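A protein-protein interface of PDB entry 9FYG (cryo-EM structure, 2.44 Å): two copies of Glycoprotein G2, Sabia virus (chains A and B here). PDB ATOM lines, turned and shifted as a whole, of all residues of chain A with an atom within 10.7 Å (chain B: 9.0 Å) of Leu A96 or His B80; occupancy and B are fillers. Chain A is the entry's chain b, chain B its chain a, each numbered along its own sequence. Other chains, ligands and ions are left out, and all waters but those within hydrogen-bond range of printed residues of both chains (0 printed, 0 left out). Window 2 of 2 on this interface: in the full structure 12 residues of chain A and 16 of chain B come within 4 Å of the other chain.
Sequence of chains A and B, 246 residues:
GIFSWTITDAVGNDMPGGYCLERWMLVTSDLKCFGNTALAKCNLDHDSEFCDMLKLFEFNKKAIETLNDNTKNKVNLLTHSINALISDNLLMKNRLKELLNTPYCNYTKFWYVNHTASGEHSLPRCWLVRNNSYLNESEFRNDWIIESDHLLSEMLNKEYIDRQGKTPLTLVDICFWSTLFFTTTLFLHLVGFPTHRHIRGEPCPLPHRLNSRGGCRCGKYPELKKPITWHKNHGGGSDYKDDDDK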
ATOM      1  N   GLU A  49      10.160  16.148 -15.988  1.00  0.00           N
ATOM      2  CA  GLU A  49       9.427  14.938 -16.333  1.00  0.00           C
ATOM      3  C   GLU A  49      10.057  13.706 -15.698  1.00  0.00           C
ATOM      4  O   GLU A  49       9.363  12.716 -15.435  1.00  0.00           O
ATOM      5  CB  GLU A  49       9.366  14.786 -17.853  1.00  0.00           C
ATOM      6  CG  GLU A  49       8.747  15.976 -18.571  1.00  0.00           C
ATOM      7  CD  GLU A  49       9.757  17.053 -18.915  1.00  0.00           C
ATOM      8  OE1 GLU A  49      10.940  16.902 -18.550  1.00  0.00           O
ATOM      9  OE2 GLU A  49       9.371  18.052 -19.550  1.00  0.00           O
ATOM     10  N   SER A  87       2.132  15.524 -13.534  1.00  0.00           N
ATOM     11  CA  SER A  87       1.657  16.887 -13.720  1.00  0.00           C
ATOM     12  C   SER A  87       0.934  16.982 -15.057  1.00  0.00           C
ATOM     13  O   SER A  87       1.542  16.781 -16.113  1.00  0.00           O
ATOM     14  CB  SER A  87       2.821  17.875 -13.663  1.00  0.00           C
ATOM     15  OG  SER A  87       2.355  19.212 -13.667  1.00  0.00           O
ATOM     16  N   ASP A  88      -0.366  17.274 -15.011  1.00  0.00           N
ATOM     17  CA  ASP A  88      -1.121  17.444 -16.247  1.00  0.00           C
ATOM     18  C   ASP A  88      -0.640  18.657 -17.031  1.00  0.00           C
ATOM     19  O   ASP A  88      -0.693  18.654 -18.264  1.00  0.00           O
ATOM     20  CB  ASP A  88      -2.615  17.563 -15.942  1.00  0.00           C
ATOM     21  CG  ASP A  88      -3.470  17.526 -17.197  1.00  0.00           C
ATOM     22  OD1 ASP A  88      -3.399  16.527 -17.941  1.00  0.00           O
ATOM     23  OD2 ASP A  88      -4.212  18.501 -17.442  1.00  0.00           O
ATOM     24  N   ASN A  89      -0.163  19.693 -16.339  1.00  0.00           N
ATOM     25  CA  ASN A  89       0.322  20.885 -17.027  1.00  0.00           C
ATOM     26  C   ASN A  89       1.603  20.601 -17.802  1.00  0.00           C
ATOM     27  O   ASN A  89       1.751  21.040 -18.946  1.00  0.00           O
ATOM     28  CB  ASN A  89       0.538  22.017 -16.023  1.00  0.00           C
ATOM     29  CG  ASN A  89      -0.765  22.578 -15.494  1.00  0.00           C
ATOM     30  OD1 ASN A  89      -1.823  22.381 -16.087  1.00  0.00           O
ATOM     31  ND2 ASN A  89      -0.694  23.280 -14.371  1.00  0.00           N
ATOM     32  N   LEU A  90       2.540  19.869 -17.195  1.00  0.00           N
ATOM     33  CA  LEU A  90       3.775  19.520 -17.888  1.00  0.00           C
ATOM     34  C   LEU A  90       3.500  18.622 -19.088  1.00  0.00           C
ATOM     35  O   LEU A  90       4.064  18.825 -20.173  1.00  0.00           O
ATOM     36  CB  LEU A  90       4.737  18.844 -16.909  1.00  0.00           C
ATOM     37  CG  LEU A  90       6.205  18.683 -17.301  1.00  0.00           C
ATOM     38  CD1 LEU A  90       6.792  20.007 -17.741  1.00  0.00           C
ATOM     39  CD2 LEU A  90       6.990  18.108 -16.140  1.00  0.00           C
ATOM     40  N   LEU A  91       2.622  17.631 -18.915  1.00  0.00           N
ATOM     41  CA  LEU A  91       2.264  16.750 -20.019  1.00  0.00           C
ATOM     42  C   LEU A  91       1.577  17.519 -21.139  1.00  0.00           C
ATOM     43  O   LEU A  91       1.851  17.286 -22.322  1.00  0.00           O
ATOM     44  CB  LEU A  91       1.368  15.619 -19.509  1.00  0.00           C
ATOM     45  CG  LEU A  91       1.236  14.370 -20.382  1.00  0.00           C
ATOM     46  CD1 LEU A  91       2.507  13.540 -20.344  1.00  0.00           C
ATOM     47  CD2 LEU A  91       0.043  13.538 -19.956  1.00  0.00           C
ATOM     48  N   MET A  92       0.680  18.441 -20.786  1.00  0.00           N
ATOM     49  CA  MET A  92      -0.006  19.240 -21.794  1.00  0.00           C
ATOM     50  C   MET A  92       0.967  20.146 -22.536  1.00  0.00           C
ATOM     51  O   MET A  92       0.871  20.300 -23.757  1.00  0.00           O
ATOM     52  CB  MET A  92      -1.124  20.054 -21.141  1.00  0.00           C
ATOM     53  CG  MET A  92      -1.737  21.117 -22.035  1.00  0.00           C
ATOM     54  SD  MET A  92      -2.627  20.417 -23.436  1.00  0.00           S
ATOM     55  CE  MET A  92      -4.018  19.659 -22.604  1.00  0.00           C
ATOM     56  N   LYS A  93       1.913  20.750 -21.813  1.00  0.00           N
ATOM     57  CA  LYS A  93       2.923  21.587 -22.450  1.00  0.00           C
ATOM     58  C   LYS A  93       3.771  20.783 -23.429  1.00  0.00           C
ATOM     59  O   LYS A  93       4.049  21.239 -24.546  1.00  0.00           O
ATOM     60  CB  LYS A  93       3.791  22.245 -21.372  1.00  0.00           C
ATOM     61  CG  LYS A  93       4.892  23.157 -21.887  1.00  0.00           C
ATOM     62  CD  LYS A  93       6.232  22.442 -21.940  1.00  0.00           C
ATOM     63  CE  LYS A  93       6.799  22.206 -20.556  1.00  0.00           C
ATOM     64  NZ  LYS A  93       8.119  21.521 -20.612  1.00  0.00           N
ATOM     65  N   ASN A  94       4.183  19.576 -23.032  1.00  0.00           N
ATOM     66  CA  ASN A  94       4.991  18.751 -23.926  1.00  0.00           C
ATOM     67  C   ASN A  94       4.191  18.297 -25.142  1.00  0.00           C
ATOM     68  O   ASN A  94       4.715  18.273 -26.262  1.00  0.00           O
ATOM     69  CB  ASN A  94       5.560  17.555 -23.165  1.00  0.00           C
ATOM     70  CG  ASN A  94       6.841  17.895 -22.431  1.00  0.00           C
ATOM     71  OD1 ASN A  94       7.776  18.436 -23.016  1.00  0.00           O
ATOM     72  ND2 ASN A  94       6.886  17.586 -21.145  1.00  0.00           N
ATOM     73  N   ARG A  95       2.916  17.948 -24.949  1.00  0.00           N
ATOM     74  CA  ARG A  95       2.082  17.566 -26.083  1.00  0.00           C
ATOM     75  C   ARG A  95       1.884  18.735 -27.041  1.00  0.00           C
ATOM     76  O   ARG A  95       1.907  18.557 -28.264  1.00  0.00           O
ATOM     77  CB  ARG A  95       0.734  17.036 -25.593  1.00  0.00           C
ATOM     78  CG  ARG A  95      -0.231  16.691 -26.710  1.00  0.00           C
ATOM     79  CD  ARG A  95       0.212  15.450 -27.465  1.00  0.00           C
ATOM     80  NE  ARG A  95      -0.388  14.235 -26.929  1.00  0.00           N
ATOM     81  CZ  ARG A  95       0.027  13.006 -27.206  1.00  0.00           C
ATOM     82  NH1 ARG A  95       1.072  12.791 -27.985  1.00  0.00           N
ATOM     83  NH2 ARG A  95      -0.620  11.970 -26.685  1.00  0.00           N
ATOM     84  N   LEU A  96       1.684  19.941 -26.503  1.00  0.00           N
ATOM     85  CA  LEU A  96       1.502  21.111 -27.353  1.00  0.00           C
ATOM     86  C   LEU A  96       2.775  21.441 -28.121  1.00  0.00           C
ATOM     87  O   LEU A  96       2.713  21.859 -29.283  1.00  0.00           O
ATOM     88  CB  LEU A  96       1.045  22.304 -26.515  1.00  0.00           C
ATOM     89  CG  LEU A  96      -0.408  22.256 -26.034  1.00  0.00           C
ATOM     90  CD1 LEU A  96      -0.764  23.513 -25.259  1.00  0.00           C
ATOM     91  CD2 LEU A  96      -1.358  22.051 -27.202  1.00  0.00           C
ATOM     92  N   LYS A  97       3.940  21.270 -27.491  1.00  0.00           N
ATOM     93  CA  LYS A  97       5.192  21.414 -28.227  1.00  0.00           C
ATOM     94  C   LYS A  97       5.310  20.366 -29.326  1.00  0.00           C
ATOM     95  O   LYS A  97       5.811  20.655 -30.418  1.00  0.00           O
ATOM     96  CB  LYS A  97       6.384  21.329 -27.276  1.00  0.00           C
ATOM     97  CG  LYS A  97       6.563  22.547 -26.396  1.00  0.00           C
ATOM     98  CD  LYS A  97       7.789  22.406 -25.518  1.00  0.00           C
ATOM     99  CE  LYS A  97       8.003  23.644 -24.670  1.00  0.00           C
ATOM    100  NZ  LYS A  97       9.206  23.514 -23.804  1.00  0.00           N
ATOM    101  N   GLU A  98       4.865  19.138 -29.052  1.00  0.00           N
ATOM    102  CA  GLU A  98       4.896  18.097 -30.074  1.00  0.00           C
ATOM    103  C   GLU A  98       4.001  18.449 -31.258  1.00  0.00           C
ATOM    104  O   GLU A  98       4.374  18.229 -32.415  1.00  0.00           O
ATOM    105  CB  GLU A  98       4.479  16.759 -29.467  1.00  0.00           C
ATOM    106  CG  GLU A  98       4.204  15.671 -30.487  1.00  0.00           C
ATOM    107  CD  GLU A  98       3.792  14.366 -29.846  1.00  0.00           C
ATOM    108  OE1 GLU A  98       3.551  14.357 -28.621  1.00  0.00           O
ATOM    109  OE2 GLU A  98       3.714  13.347 -30.563  1.00  0.00           O
ATOM    110  N   LEU A  99       2.815  18.999 -30.987  1.00  0.00           N
ATOM    111  CA  LEU A  99       1.881  19.330 -32.058  1.00  0.00           C
ATOM    112  C   LEU A  99       2.371  20.474 -32.934  1.00  0.00           C
ATOM    113  O   LEU A  99       1.956  20.570 -34.094  1.00  0.00           O
ATOM    114  CB  LEU A  99       0.509  19.677 -31.475  1.00  0.00           C
ATOM    115  CG  LEU A  99      -0.198  18.562 -30.703  1.00  0.00           C
ATOM    116  CD1 LEU A  99      -1.467  19.074 -30.046  1.00  0.00           C
ATOM    117  CD2 LEU A  99      -0.496  17.383 -31.612  1.00  0.00           C
ATOM    118  N   LEU A 100       3.242  21.336 -32.416  1.00  0.00           N
ATOM    119  CA  LEU A 100       3.751  22.482 -33.155  1.00  0.00           C
ATOM    120  C   LEU A 100       5.104  22.214 -33.804  1.00  0.00           C
ATOM    121  O   LEU A 100       5.739  23.154 -34.290  1.00  0.00           O
ATOM    122  CB  LEU A 100       3.844  23.701 -32.238  1.00  0.00           C
ATOM    123  CG  LEU A 100       2.525  24.173 -31.629  1.00  0.00           C
ATOM    124  CD1 LEU A 100       2.782  25.142 -30.490  1.00  0.00           C
ATOM    125  CD2 LEU A 100       1.645  24.806 -32.691  1.00  0.00           C
ATOM    126  N   ASN A 101       5.558  20.960 -33.808  1.00  0.00           N
ATOM    127  CA  ASN A 101       6.814  20.557 -34.448  1.00  0.00           C
ATOM    128  C   ASN A 101       8.025  21.246 -33.824  1.00  0.00           C
ATOM    129  O   ASN A 101       9.006  21.545 -34.509  1.00  0.00           O
ATOM    130  CB  ASN A 101       6.773  20.806 -35.959  1.00  0.00           C
ATOM    131  CG  ASN A 101       5.956  19.766 -36.694  1.00  0.00           C
ATOM    132  OD1 ASN A 101       4.998  20.092 -37.394  1.00  0.00           O
ATOM    133  ND2 ASN A 101       6.326  18.500 -36.535  1.00  0.00           N
ATOM    134  N   THR A 102       7.965  21.493 -32.535  1.00  0.00           N
ATOM    135  CA  THR A 102       8.923  22.009 -31.574  1.00  0.00           C
ATOM    136  C   THR A 102       9.527  20.855 -30.780  1.00  0.00           C
ATOM    137  O   THR A 102       8.846  19.859 -30.520  1.00  0.00           O
ATOM    138  CB  THR A 102       8.233  22.996 -30.623  1.00  0.00           C
ATOM    139  OG1 THR A 102       7.651  24.062 -31.383  1.00  0.00           O
ATOM    140  CG2 THR A 102       9.202  23.584 -29.609  1.00  0.00           C
ATOM    141  N   PRO A 103      10.808  20.923 -30.407  1.00  0.00           N
ATOM    142  CA  PRO A 103      11.374  19.871 -29.552  1.00  0.00           C
ATOM    143  C   PRO A 103      10.582  19.727 -28.260  1.00  0.00           C
ATOM    144  O   PRO A 103      10.185  20.713 -27.638  1.00  0.00           O
ATOM    145  CB  PRO A 103      12.801  20.358 -29.290  1.00  0.00           C
ATOM    146  CG  PRO A 103      13.130  21.192 -30.466  1.00  0.00           C
ATOM    147  CD  PRO A 103      11.849  21.827 -30.930  1.00  0.00           C
ATOM    148  N   TYR A 104      10.360  18.478 -27.861  1.00  0.00           N
ATOM    149  CA  TYR A 104       9.457  18.181 -26.762  1.00  0.00           C
ATOM    150  C   TYR A 104       9.932  16.927 -26.046  1.00  0.00           C
ATOM    151  O   TYR A 104      10.737  16.153 -26.568  1.00  0.00           O
ATOM    152  CB  TYR A 104       8.013  18.000 -27.252  1.00  0.00           C
ATOM    153  CG  TYR A 104       7.797  16.732 -28.048  1.00  0.00           C
ATOM    154  CD1 TYR A 104       8.147  16.664 -29.389  1.00  0.00           C
ATOM    155  CD2 TYR A 104       7.251  15.602 -27.457  1.00  0.00           C
ATOM    156  CE1 TYR A 104       7.959  15.509 -30.117  1.00  0.00           C
ATOM    157  CE2 TYR A 104       7.062  14.444 -28.177  1.00  0.00           C
ATOM    158  CZ  TYR A 104       7.416  14.403 -29.507  1.00  0.00           C
ATOM    159  OH  TYR A 104       7.225  13.251 -30.232  1.00  0.00           O
ATOM    160  N   CYS A 105       9.411  16.735 -24.839  1.00  0.00           N
ATOM    161  CA  CYS A 105       9.712  15.558 -24.038  1.00  0.00           C
ATOM    162  C   CYS A 105       8.635  14.506 -24.267  1.00  0.00           C
ATOM    163  O   CYS A 105       7.446  14.778 -24.073  1.00  0.00           O
ATOM    164  CB  CYS A 105       9.798  15.921 -22.557  1.00  0.00           C
ATOM    165  SG  CYS A 105      10.242  14.543 -21.487  1.00  0.00           S
ATOM    166  N   ASN A 106       9.047  13.305 -24.677  1.00  0.00           N
ATOM    167  CA  ASN A 106       8.120  12.191 -24.814  1.00  0.00           C
ATOM    168  C   ASN A 106       8.319  11.147 -23.716  1.00  0.00           C
ATOM    169  O   ASN A 106       7.908   9.992 -23.870  1.00  0.00           O
ATOM    170  CB  ASN A 106       8.201  11.601 -26.230  1.00  0.00           C
ATOM    171  CG  ASN A 106       9.325  10.592 -26.428  1.00  0.00           C
ATOM    172  OD1 ASN A 106      10.300  10.536 -25.683  1.00  0.00           O
ATOM    173  ND2 ASN A 106       9.177   9.787 -27.477  1.00  0.00           N
ATOM    174  N   TYR A 107       8.943  11.551 -22.604  1.00  0.00           N
ATOM    175  CA  TYR A 107       8.916  10.828 -21.330  1.00  0.00           C
ATOM    176  C   TYR A 107       9.571   9.454 -21.419  1.00  0.00           C
ATOM    177  O   TYR A 107       9.196   8.529 -20.696  1.00  0.00           O
ATOM    178  CB  TYR A 107       7.484  10.703 -20.800  1.00  0.00           C
ATOM    179  CG  TYR A 107       6.891  12.011 -20.322  1.00  0.00           C
ATOM    180  CD1 TYR A 107       6.498  12.990 -21.225  1.00  0.00           C
ATOM    181  CD2 TYR A 107       6.730  12.268 -18.970  1.00  0.00           C
ATOM    182  CE1 TYR A 107       5.963  14.184 -20.794  1.00  0.00           C
ATOM    183  CE2 TYR A 107       6.191  13.456 -18.527  1.00  0.00           C
ATOM    184  CZ  TYR A 107       5.810  14.412 -19.444  1.00  0.00           C
ATOM    185  OH  TYR A 107       5.277  15.600 -19.005  1.00  0.00           O
ATOM    186  N   VAL A 129      12.848  15.479 -28.490  1.00  0.00           N
ATOM    187  CA  VAL A 129      12.533  14.749 -29.712  1.00  0.00           C
ATOM    188  C   VAL A 129      12.015  15.731 -30.755  1.00  0.00           C
ATOM    189  O   VAL A 129      11.220  16.624 -30.438  1.00  0.00           O
ATOM    190  CB  VAL A 129      11.491  13.639 -29.449  1.00  0.00           C
ATOM    191  CG1 VAL A 129      10.963  13.063 -30.756  1.00  0.00           C
ATOM    192  CG2 VAL A 129      12.083  12.547 -28.583  1.00  0.00           C
ATOM    193  N   PHE B  59       4.109  32.838 -24.234  1.00  0.00           N
ATOM    194  CA  PHE B  59       3.283  31.956 -25.052  1.00  0.00           C
ATOM    195  C   PHE B  59       2.677  32.712 -26.230  1.00  0.00           C
ATOM    196  O   PHE B  59       2.695  32.232 -27.369  1.00  0.00           O
ATOM    197  CB  PHE B  59       2.190  31.321 -24.192  1.00  0.00           C
ATOM    198  CG  PHE B  59       1.480  30.176 -24.856  1.00  0.00           C
ATOM    199  CD1 PHE B  59       1.946  28.880 -24.715  1.00  0.00           C
ATOM    200  CD2 PHE B  59       0.346  30.393 -25.617  1.00  0.00           C
ATOM    201  CE1 PHE B  59       1.298  27.827 -25.326  1.00  0.00           C
ATOM    202  CE2 PHE B  59      -0.307  29.345 -26.230  1.00  0.00           C
ATOM    203  CZ  PHE B  59       0.170  28.061 -26.086  1.00  0.00           C
ATOM    204  N   LYS B  62       5.525  33.538 -28.853  1.00  0.00           N
ATOM    205  CA  LYS B  62       5.923  32.383 -29.649  1.00  0.00           C
ATOM    206  C   LYS B  62       4.786  31.857 -30.514  1.00  0.00           C
ATOM    207  O   LYS B  62       5.049  31.168 -31.505  1.00  0.00           O
ATOM    208  CB  LYS B  62       6.471  31.277 -28.743  1.00  0.00           C
ATOM    209  CG  LYS B  62       5.431  30.515 -27.952  1.00  0.00           C
ATOM    210  CD  LYS B  62       6.096  29.675 -26.873  1.00  0.00           C
ATOM    211  CE  LYS B  62       5.100  28.766 -26.178  1.00  0.00           C
ATOM    212  NZ  LYS B  62       5.657  28.202 -24.917  1.00  0.00           N
ATOM    213  N   VAL B  75      -4.025  28.146 -35.814  1.00  0.00           N
ATOM    214  CA  VAL B  75      -4.815  27.649 -34.694  1.00  0.00           C
ATOM    215  C   VAL B  75      -4.279  28.266 -33.411  1.00  0.00           C
ATOM    216  O   VAL B  75      -3.072  28.211 -33.145  1.00  0.00           O
ATOM    217  CB  VAL B  75      -4.779  26.112 -34.620  1.00  0.00           C
ATOM    218  CG1 VAL B  75      -5.328  25.625 -33.288  1.00  0.00           C
ATOM    219  CG2 VAL B  75      -5.560  25.509 -35.777  1.00  0.00           C
ATOM    220  N   ASN B  76      -5.173  28.857 -32.622  1.00  0.00           N
ATOM    221  CA  ASN B  76      -4.821  29.396 -31.317  1.00  0.00           C
ATOM    222  C   ASN B  76      -4.936  28.296 -30.270  1.00  0.00           C
ATOM    223  O   ASN B  76      -5.963  27.616 -30.183  1.00  0.00           O
ATOM    224  CB  ASN B  76      -5.731  30.572 -30.955  1.00  0.00           C
ATOM    225  CG  ASN B  76      -4.990  31.688 -30.249  1.00  0.00           C
ATOM    226  OD1 ASN B  76      -4.327  31.466 -29.238  1.00  0.00           O
ATOM    227  ND2 ASN B  76      -5.104  32.898 -30.779  1.00  0.00           N
ATOM    228  N   LEU B  77      -3.876  28.120 -29.481  1.00  0.00           N
ATOM    229  CA  LEU B  77      -3.824  27.078 -28.465  1.00  0.00           C
ATOM    230  C   LEU B  77      -3.846  27.647 -27.052  1.00  0.00           C
ATOM    231  O   LEU B  77      -3.452  26.959 -26.107  1.00  0.00           O
ATOM    232  CB  LEU B  77      -2.582  26.209 -28.667  1.00  0.00           C
ATOM    233  CG  LEU B  77      -2.523  25.380 -29.952  1.00  0.00           C
ATOM    234  CD1 LEU B  77      -1.249  24.557 -29.998  1.00  0.00           C
ATOM    235  CD2 LEU B  77      -3.741  24.487 -30.068  1.00  0.00           C
ATOM    236  N   LEU B  78      -4.300  28.893 -26.891  1.00  0.00           N
ATOM    237  CA  LEU B  78      -4.254  29.536 -25.582  1.00  0.00           C
ATOM    238  C   LEU B  78      -5.168  28.850 -24.571  1.00  0.00           C
ATOM    239  O   LEU B  78      -4.834  28.790 -23.384  1.00  0.00           O
ATOM    240  CB  LEU B  78      -4.619  31.016 -25.709  1.00  0.00           C
ATOM    241  CG  LEU B  78      -4.418  31.876 -24.459  1.00  0.00           C
ATOM    242  CD1 LEU B  78      -3.061  31.612 -23.828  1.00  0.00           C
ATOM    243  CD2 LEU B  78      -4.586  33.348 -24.783  1.00  0.00           C
ATOM    244  N   THR B  79      -6.318  28.337 -25.011  1.00  0.00           N
ATOM    245  CA  THR B  79      -7.221  27.658 -24.089  1.00  0.00           C
ATOM    246  C   THR B  79      -6.680  26.313 -23.623  1.00  0.00           C
ATOM    247  O   THR B  79      -7.089  25.830 -22.563  1.00  0.00           O
ATOM    248  CB  THR B  79      -8.596  27.468 -24.729  1.00  0.00           C
ATOM    249  OG1 THR B  79      -8.470  26.696 -25.929  1.00  0.00           O
ATOM    250  CG2 THR B  79      -9.218  28.814 -25.055  1.00  0.00           C
ATOM    251  N   HIS B  80      -5.776  25.699 -24.387  1.00  0.00           N
ATOM    252  CA  HIS B  80      -5.184  24.434 -23.972  1.00  0.00           C
ATOM    253  C   HIS B  80      -4.124  24.619 -22.896  1.00  0.00           C
ATOM    254  O   HIS B  80      -3.899  23.707 -22.094  1.00  0.00           O
ATOM    255  CB  HIS B  80      -4.576  23.717 -25.178  1.00  0.00           C
ATOM    256  CG  HIS B  80      -5.590  23.242 -26.169  1.00  0.00           C
ATOM    257  ND1 HIS B  80      -6.533  22.285 -25.867  1.00  0.00           N
ATOM    258  CD2 HIS B  80      -5.812  23.597 -27.455  1.00  0.00           C
ATOM    259  CE1 HIS B  80      -7.290  22.068 -26.927  1.00  0.00           C
ATOM    260  NE2 HIS B  80      -6.875  22.852 -27.903  1.00  0.00           N
ATOM    261  N   SER B  81      -3.469  25.779 -22.858  1.00  0.00           N
ATOM    262  CA  SER B  81      -2.362  26.014 -21.941  1.00  0.00           C
ATOM    263  C   SER B  81      -2.639  27.126 -20.938  1.00  0.00           C
ATOM    264  O   SER B  81      -1.730  27.506 -20.191  1.00  0.00           O
ATOM    265  CB  SER B  81      -1.089  26.336 -22.726  1.00  0.00           C
ATOM    266  OG  SER B  81      -1.249  27.537 -23.455  1.00  0.00           O
ATOM    267  N   ILE B  82      -3.862  27.661 -20.900  1.00  0.00           N
ATOM    268  CA  ILE B  82      -4.164  28.737 -19.962  1.00  0.00           C
ATOM    269  C   ILE B  82      -4.016  28.262 -18.521  1.00  0.00           C
ATOM    270  O   ILE B  82      -3.618  29.036 -17.644  1.00  0.00           O
ATOM    271  CB  ILE B  82      -5.568  29.319 -20.246  1.00  0.00           C
ATOM    272  CG1 ILE B  82      -5.773  30.628 -19.479  1.00  0.00           C
ATOM    273  CG2 ILE B  82      -6.669  28.316 -19.928  1.00  0.00           C
ATOM    274  CD1 ILE B  82      -5.012  31.793 -20.057  1.00  0.00           C
ATOM    275  N   ASN B  83      -4.323  26.989 -18.251  1.00  0.00           N
ATOM    276  CA  ASN B  83      -4.083  26.436 -16.923  1.00  0.00           C
ATOM    277  C   ASN B  83      -2.593  26.369 -16.609  1.00  0.00           C
ATOM    278  O   ASN B  83      -2.176  26.650 -15.480  1.00  0.00           O
ATOM    279  CB  ASN B  83      -4.715  25.051 -16.806  1.00  0.00           C
ATOM    280  CG  ASN B  83      -6.167  25.106 -16.386  1.00  0.00           C
ATOM    281  OD1 ASN B  83      -6.526  25.814 -15.447  1.00  0.00           O
ATOM    282  ND2 ASN B  83      -7.013  24.357 -17.081  1.00  0.00           N
ATOM    283  N   ALA B  84      -1.777  25.994 -17.594  1.00  0.00           N
ATOM    284  CA  ALA B  84      -0.342  25.886 -17.362  1.00  0.00           C
ATOM    285  C   ALA B  84       0.313  27.251 -17.199  1.00  0.00           C
ATOM    286  O   ALA B  84       1.347  27.362 -16.531  1.00  0.00           O
ATOM    287  CB  ALA B  84       0.320  25.114 -18.503  1.00  0.00           C
ATOM    288  N   LEU B  85      -0.258  28.293 -17.798  1.00  0.00           N
ATOM    289  CA  LEU B  85       0.334  29.624 -17.705  1.00  0.00           C
ATOM    290  C   LEU B  85      -0.226  30.436 -16.545  1.00  0.00           C
ATOM    291  O   LEU B  85       0.511  31.196 -15.910  1.00  0.00           O
ATOM    292  CB  LEU B  85       0.131  30.389 -19.015  1.00  0.00           C
ATOM    293  CG  LEU B  85       0.532  29.669 -20.303  1.00  0.00           C
ATOM    294  CD1 LEU B  85      -0.091  30.352 -21.510  1.00  0.00           C
ATOM    295  CD2 LEU B  85       2.044  29.593 -20.440  1.00  0.00           C
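No position is printed for both chains.
Of the 7 pairs that touch across the chains among the printed residues, none has its exchanged pair printed and touching as well.
Asn A89 touches Asn B83 (ND2 to O, 3.8 Å).
Asn A89 touches Ala B84.
Leu A96 touches Leu B77.
Leu A96 touches His B80 (CD1 to CB, 3.8 Å).
Ser B81 touches Leu A96 (CB to CD1, 3.8 Å).
Leu B77 touches Leu A100.
The backbone carbonyl oxygen (O) of His B80 lies close to the side-chain sulfur (SD) of Met A92, at 3.8 Å.
O of Leu B77 lies within hydrogen-bond range of OG of Ser B81 (3.5 Å).
Of the 13 printed residues of chain B, 5 touch a printed residue of chain A.
Hydrophobic or aromatic side chains of chain B within 4 Å of the printed part of chain A: Leu B77, His B80 and Ala B84.
Hydrophobic or aromatic side chains of chain A that line the printed part of chain B: Met A92, Leu A96 and Leu A100.
Among the printed residues, 7 pairs touch across the chains.
Among the printed residues, no Asp or Glu carboxylate lies within 4 Å of a Lys or Arg side-chain nitrogen of the other chain.
Printed residues of chain B within 4 Å of Asn A89: Asn B83 and Ala B84.
Of the printed residues of chain B, Met A92 touches His B80.
Leu A96 touches three residues of chain B.
Lys A97 touches none of the printed residues of chain B.
Of the printed residues of chain B, Leu A100 touches Leu B77.
Val A129 touches none of the printed residues of chain B.
Of chain A, only Leu A96 (3.8 Å) and Leu A100 (3.96 Å) come within 4 Å of Leu B77.
Thr B79 touches none of the printed residues of chain A.
Ser B81 touches just one residue of chain A: Leu A96.
Of the printed residues of chain A, Asn B83 touches Asn A89.
Of the printed residues of chain A, Ala B84 touches Asn A89.
The nearest printed residue of chain B that does not touch Asn A89 is Leu B85 (6.1 Å).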
